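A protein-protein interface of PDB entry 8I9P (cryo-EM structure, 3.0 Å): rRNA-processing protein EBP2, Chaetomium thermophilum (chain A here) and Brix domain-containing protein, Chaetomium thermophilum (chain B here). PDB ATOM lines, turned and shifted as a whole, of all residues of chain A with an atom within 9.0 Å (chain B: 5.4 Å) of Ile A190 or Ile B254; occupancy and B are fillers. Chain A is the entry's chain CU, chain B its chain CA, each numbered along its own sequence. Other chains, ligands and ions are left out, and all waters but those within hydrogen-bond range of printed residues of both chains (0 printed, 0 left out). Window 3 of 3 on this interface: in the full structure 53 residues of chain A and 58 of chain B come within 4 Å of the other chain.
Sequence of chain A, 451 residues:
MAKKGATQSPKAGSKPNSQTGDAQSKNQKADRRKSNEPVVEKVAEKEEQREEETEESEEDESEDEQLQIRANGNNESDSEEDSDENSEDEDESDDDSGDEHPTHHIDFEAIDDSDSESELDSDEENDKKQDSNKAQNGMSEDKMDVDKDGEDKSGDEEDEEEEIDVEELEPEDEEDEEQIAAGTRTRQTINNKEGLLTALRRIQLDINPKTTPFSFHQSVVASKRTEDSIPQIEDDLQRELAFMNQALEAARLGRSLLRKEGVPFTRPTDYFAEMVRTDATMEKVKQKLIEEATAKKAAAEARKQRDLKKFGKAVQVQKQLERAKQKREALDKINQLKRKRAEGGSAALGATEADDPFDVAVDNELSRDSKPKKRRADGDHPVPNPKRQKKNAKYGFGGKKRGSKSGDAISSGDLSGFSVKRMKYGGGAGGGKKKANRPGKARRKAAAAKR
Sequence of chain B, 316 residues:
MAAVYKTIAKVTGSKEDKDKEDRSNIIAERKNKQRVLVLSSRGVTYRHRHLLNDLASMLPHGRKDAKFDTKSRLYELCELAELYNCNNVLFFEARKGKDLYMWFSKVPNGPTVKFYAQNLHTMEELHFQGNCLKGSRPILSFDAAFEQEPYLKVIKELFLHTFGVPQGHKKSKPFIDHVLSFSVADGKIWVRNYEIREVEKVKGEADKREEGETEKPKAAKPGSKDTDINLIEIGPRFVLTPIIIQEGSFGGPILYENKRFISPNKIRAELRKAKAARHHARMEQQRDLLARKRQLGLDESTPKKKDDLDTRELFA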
ATOM      1  N   ILE A 190      14.179  10.867   5.925  1.00  0.00           N
ATOM      2  CA  ILE A 190      15.275  11.611   5.324  1.00  0.00           C
ATOM      3  C   ILE A 190      15.689  10.956   4.012  1.00  0.00           C
ATOM      4  O   ILE A 190      15.399   9.783   3.771  1.00  0.00           O
ATOM      5  CB  ILE A 190      16.464  11.725   6.299  1.00  0.00           C
ATOM      6  CG1 ILE A 190      17.305  10.447   6.288  1.00  0.00           C
ATOM      7  CG2 ILE A 190      15.968  12.024   7.705  1.00  0.00           C
ATOM      8  CD1 ILE A 190      18.520  10.506   7.186  1.00  0.00           C
ATOM      9  N   ASN A 191      16.346  11.732   3.148  1.00  0.00           N
ATOM     10  CA  ASN A 191      16.853  11.231   1.867  1.00  0.00           C
ATOM     11  C   ASN A 191      18.299  11.703   1.729  1.00  0.00           C
ATOM     12  O   ASN A 191      18.569  12.737   1.112  1.00  0.00           O
ATOM     13  CB  ASN A 191      15.992  11.701   0.703  1.00  0.00           C
ATOM     14  CG  ASN A 191      14.799  10.802   0.461  1.00  0.00           C
ATOM     15  OD1 ASN A 191      13.949  10.632   1.334  1.00  0.00           O
ATOM     16  ND2 ASN A 191      14.729  10.219  -0.729  1.00  0.00           N
ATOM     17  N   ASN A 192      19.223  10.939   2.304  1.00  0.00           N
ATOM     18  CA  ASN A 192      20.653  11.205   2.153  1.00  0.00           C
ATOM     19  C   ASN A 192      21.086  10.577   0.838  1.00  0.00           C
ATOM     20  O   ASN A 192      21.587   9.452   0.800  1.00  0.00           O
ATOM     21  CB  ASN A 192      21.438  10.648   3.333  1.00  0.00           C
ATOM     22  CG  ASN A 192      22.861  11.158   3.373  1.00  0.00           C
ATOM     23  OD1 ASN A 192      23.216  12.091   2.655  1.00  0.00           O
ATOM     24  ND2 ASN A 192      23.686  10.549   4.216  1.00  0.00           N
ATOM     25  N   LYS A 193      20.894  11.332  -0.251  1.00  0.00           N
ATOM     26  CA  LYS A 193      20.973  10.770  -1.598  1.00  0.00           C
ATOM     27  C   LYS A 193      22.372  10.265  -1.928  1.00  0.00           C
ATOM     28  O   LYS A 193      22.526   9.148  -2.440  1.00  0.00           O
ATOM     29  CB  LYS A 193      20.530  11.815  -2.623  1.00  0.00           C
ATOM     30  CG  LYS A 193      19.083  12.256  -2.478  1.00  0.00           C
ATOM     31  CD  LYS A 193      18.659  13.157  -3.627  1.00  0.00           C
ATOM     32  CE  LYS A 193      17.197  13.554  -3.506  1.00  0.00           C
ATOM     33  NZ  LYS A 193      16.762  14.430  -4.629  1.00  0.00           N
ATOM     34  N   GLY A 195      24.614   9.206   0.000  1.00  0.00           N
ATOM     35  CA  GLY A 195      24.805   7.945   0.696  1.00  0.00           C
ATOM     36  C   GLY A 195      24.231   6.770  -0.069  1.00  0.00           C
ATOM     37  O   GLY A 195      24.838   5.696  -0.121  1.00  0.00           O
ATOM     38  N   LEU A 196      23.067   6.958  -0.697  1.00  0.00           N
ATOM     39  CA  LEU A 196      22.482   5.872  -1.470  1.00  0.00           C
ATOM     40  C   LEU A 196      23.286   5.599  -2.736  1.00  0.00           C
ATOM     41  O   LEU A 196      23.486   4.434  -3.106  1.00  0.00           O
ATOM     42  CB  LEU A 196      21.022   6.171  -1.806  1.00  0.00           C
ATOM     43  CG  LEU A 196      20.085   6.088  -0.596  1.00  0.00           C
ATOM     44  CD1 LEU A 196      19.356   7.405  -0.358  1.00  0.00           C
ATOM     45  CD2 LEU A 196      19.119   4.922  -0.694  1.00  0.00           C
ATOM     46  N   ILE B 244      12.024   1.816   5.179  1.00  0.00           N
ATOM     47  CA  ILE B 244      13.357   2.430   5.468  1.00  0.00           C
ATOM     48  C   ILE B 244      14.472   1.734   4.684  1.00  0.00           C
ATOM     49  O   ILE B 244      14.317   0.539   4.368  1.00  0.00           O
ATOM     50  CB  ILE B 244      13.681   2.437   6.978  1.00  0.00           C
ATOM     51  CG1 ILE B 244      13.348   1.101   7.649  1.00  0.00           C
ATOM     52  CG2 ILE B 244      13.010   3.608   7.678  1.00  0.00           C
ATOM     53  CD1 ILE B 244      14.556   0.373   8.190  1.00  0.00           C
ATOM     54  N   ILE B 245      15.547   2.466   4.381  1.00  0.00           N
ATOM     55  CA  ILE B 245      16.738   1.860   3.714  1.00  0.00           C
ATOM     56  C   ILE B 245      17.952   2.212   4.573  1.00  0.00           C
ATOM     57  O   ILE B 245      18.245   3.409   4.708  1.00  0.00           O
ATOM     58  CB  ILE B 245      16.903   2.343   2.259  1.00  0.00           C
ATOM     59  CG1 ILE B 245      15.703   1.962   1.389  1.00  0.00           C
ATOM     60  CG2 ILE B 245      18.207   1.831   1.666  1.00  0.00           C
ATOM     61  CD1 ILE B 245      15.855   2.346  -0.062  1.00  0.00           C
ATOM     62  N   GLN B 246      18.603   1.208   5.160  1.00  0.00           N
ATOM     63  CA  GLN B 246      19.764   1.429   6.008  1.00  0.00           C
ATOM     64  C   GLN B 246      21.055   1.152   5.245  1.00  0.00           C
ATOM     65  O   GLN B 246      21.069   0.506   4.194  1.00  0.00           O
ATOM     66  CB  GLN B 246      19.711   0.539   7.248  1.00  0.00           C
ATOM     67  CG  GLN B 246      18.470   0.686   8.089  1.00  0.00           C
ATOM     68  CD  GLN B 246      18.285  -0.471   9.049  1.00  0.00           C
ATOM     69  OE1 GLN B 246      17.992  -1.593   8.637  1.00  0.00           O
ATOM     70  NE2 GLN B 246      18.461  -0.206  10.337  1.00  0.00           N
ATOM     71  N   GLU B 247      22.158   1.630   5.815  1.00  0.00           N
ATOM     72  CA  GLU B 247      23.492   1.450   5.256  1.00  0.00           C
ATOM     73  C   GLU B 247      24.166   0.168   5.725  1.00  0.00           C
ATOM     74  O   GLU B 247      24.863  -0.481   4.939  1.00  0.00           O
ATOM     75  CB  GLU B 247      24.373   2.651   5.616  1.00  0.00           C
ATOM     76  CG  GLU B 247      25.655   2.754   4.812  1.00  0.00           C
ATOM     77  CD  GLU B 247      26.802   3.316   5.624  1.00  0.00           C
ATOM     78  OE1 GLU B 247      27.105   2.751   6.696  1.00  0.00           O
ATOM     79  OE2 GLU B 247      27.400   4.324   5.193  1.00  0.00           O
ATOM     80  N   GLY B 252      23.284   0.156  11.289  1.00  0.00           N
ATOM     81  CA  GLY B 252      23.913   1.258  10.606  1.00  0.00           C
ATOM     82  C   GLY B 252      23.000   2.462  10.511  1.00  0.00           C
ATOM     83  O   GLY B 252      21.843   2.429  10.943  1.00  0.00           O
ATOM     84  N   PRO B 253      23.508   3.553   9.942  1.00  0.00           N
ATOM     85  CA  PRO B 253      22.705   4.774   9.845  1.00  0.00           C
ATOM     86  C   PRO B 253      21.568   4.628   8.850  1.00  0.00           C
ATOM     87  O   PRO B 253      21.635   3.847   7.897  1.00  0.00           O
ATOM     88  CB  PRO B 253      23.719   5.821   9.375  1.00  0.00           C
ATOM     89  CG  PRO B 253      24.708   5.023   8.597  1.00  0.00           C
ATOM     90  CD  PRO B 253      24.845   3.729   9.350  1.00  0.00           C
ATOM     91  N   ILE B 254      20.509   5.391   9.086  1.00  0.00           N
ATOM     92  CA  ILE B 254      19.367   5.409   8.183  1.00  0.00           C
ATOM     93  C   ILE B 254      19.716   6.260   6.971  1.00  0.00           C
ATOM     94  O   ILE B 254      20.135   7.417   7.102  1.00  0.00           O
ATOM     95  CB  ILE B 254      18.114   5.934   8.909  1.00  0.00           C
ATOM     96  CG1 ILE B 254      17.473   4.816   9.738  1.00  0.00           C
ATOM     97  CG2 ILE B 254      17.104   6.522   7.923  1.00  0.00           C
ATOM     98  CD1 ILE B 254      16.622   3.856   8.935  1.00  0.00           C
ATOM     99  N   LEU B 255      19.566   5.681   5.783  1.00  0.00           N
ATOM    100  CA  LEU B 255      19.802   6.400   4.538  1.00  0.00           C
ATOM    101  C   LEU B 255      18.514   6.921   3.926  1.00  0.00           C
ATOM    102  O   LEU B 255      18.462   8.077   3.492  1.00  0.00           O
ATOM    103  CB  LEU B 255      20.532   5.497   3.532  1.00  0.00           C
ATOM    104  CG  LEU B 255      22.005   5.210   3.823  1.00  0.00           C
ATOM    105  CD1 LEU B 255      22.598   4.329   2.739  1.00  0.00           C
ATOM    106  CD2 LEU B 255      22.790   6.504   3.957  1.00  0.00           C
ATOM    107  N   TYR B 256      17.471   6.100   3.880  1.00  0.00           N
ATOM    108  CA  TYR B 256      16.167   6.511   3.382  1.00  0.00           C
ATOM    109  C   TYR B 256      15.099   6.211   4.421  1.00  0.00           C
ATOM    110  O   TYR B 256      15.033   5.098   4.949  1.00  0.00           O
ATOM    111  CB  TYR B 256      15.822   5.803   2.071  1.00  0.00           C
ATOM    112  CG  TYR B 256      14.423   6.090   1.579  1.00  0.00           C
ATOM    113  CD1 TYR B 256      14.008   7.390   1.325  1.00  0.00           C
ATOM    114  CD2 TYR B 256      13.514   5.059   1.376  1.00  0.00           C
ATOM    115  CE1 TYR B 256      12.727   7.656   0.876  1.00  0.00           C
ATOM    116  CE2 TYR B 256      12.232   5.315   0.927  1.00  0.00           C
ATOM    117  CZ  TYR B 256      11.844   6.615   0.678  1.00  0.00           C
ATOM    118  OH  TYR B 256      10.569   6.874   0.232  1.00  0.00           O
ATOM    119  N   GLU B 257      14.260   7.205   4.702  1.00  0.00           N
ATOM    120  CA  GLU B 257      13.115   7.047   5.589  1.00  0.00           C
ATOM    121  C   GLU B 257      11.878   7.570   4.876  1.00  0.00           C
ATOM    122  O   GLU B 257      11.869   8.711   4.402  1.00  0.00           O
ATOM    123  CB  GLU B 257      13.327   7.787   6.913  1.00  0.00           C
ATOM    124  CG  GLU B 257      12.062   7.966   7.732  1.00  0.00           C
ATOM    125  CD  GLU B 257      12.235   7.528   9.170  1.00  0.00           C
ATOM    126  OE1 GLU B 257      13.339   7.721   9.720  1.00  0.00           O
ATOM    127  OE2 GLU B 257      11.269   6.993   9.751  1.00  0.00           O
ATOM    128  N   LYS B 259       8.558   9.094   5.052  1.00  0.00           N
ATOM    129  CA  LYS B 259       7.638   9.835   5.917  1.00  0.00           C
ATOM    130  C   LYS B 259       6.256   9.967   5.283  1.00  0.00           C
ATOM    131  O   LYS B 259       5.697  11.056   5.161  1.00  0.00           O
ATOM    132  CB  LYS B 259       8.219  11.202   6.258  1.00  0.00           C
ATOM    133  CG  LYS B 259       9.312  11.688   5.321  1.00  0.00           C
ATOM    134  CD  LYS B 259      10.233  12.668   6.034  1.00  0.00           C
ATOM    135  CE  LYS B 259      11.554  12.833   5.302  1.00  0.00           C
ATOM    136  NZ  LYS B 259      12.456  13.805   5.979  1.00  0.00           N
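The backbone carbonyl oxygen of Ile A190 lies within hydrogen-bond range of the backbone NH of Glu B257, 3.0 Å away.
N of Asn A192 is in hydrogen-bond range of O of Leu B255 (3.2 Å).
The backbone NH (N) of Ile A190 lies close to the side-chain amino group (NZ) of Lys B259, at 3.4 Å.
The backbone carbonyl oxygen of Ile B245 is in hydrogen-bond range of the backbone NH of Leu B255, 2.8 Å away.
The backbone carbonyl oxygen of Tyr B256 is in hydrogen-bond range of the backbone NH of Ile B245, 2.7 Å away.
Among the printed residues, merely in contact across the chains: Asn A191 with Tyr B256 (3.2 Å), Ile A190 with Tyr B256 (3.4 Å), Ile A190 with Ile B254 (3.5 Å), Ile A190 with Leu B255 (3.5 Å), Gly A195 with Leu B255 (3.9 Å), Asn A191 with Leu B255 (3.9 Å) and Leu A196 with Ile B245 (3.99 Å).
Ile A190 touches just these residues of chain B: Ile B254, Leu B255, Tyr B256, Glu B257 and Lys B259.
Of chain A, only Ile A190 comes within 4 Å of Ile B254.
No residue of chain A comes within 4 Å of Pro B253.
Of the printed residues of chain A, Lys B259 touches Ile A190.
Of the printed residues of chain A, Glu B257 touches Ile A190 (3.0 Å).
Of the printed residues of chain A, Leu B255 touches Ile A190 (3.5 Å), Asn A191 (3.9 Å), Asn A192 (3.2 Å) and Gly A195 (3.9 Å).
The nearest printed residue of chain B that does not touch Ile A190 is Pro B253 (6.8 Å).
The nearest residue of chain A that does not touch Ile B254 is Asn A192 (5.1 Å).
The nearest printed residue of chain A that does not touch Lys B259 is Asn A191 (5.1 Å).
Hydrophobic or aromatic side chains of chain A within 4 Å of the printed part of chain B: Ile A190 and Leu A196.
Of the 11 printed residues of chain B, 6 touch a printed residue of chain A.
Among the printed residues, 10 pairs touch across the chains.
Among the printed residues, no Asp or Glu carboxylate lies within 4 Å of a Lys or Arg side-chain nitrogen of the other chain.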
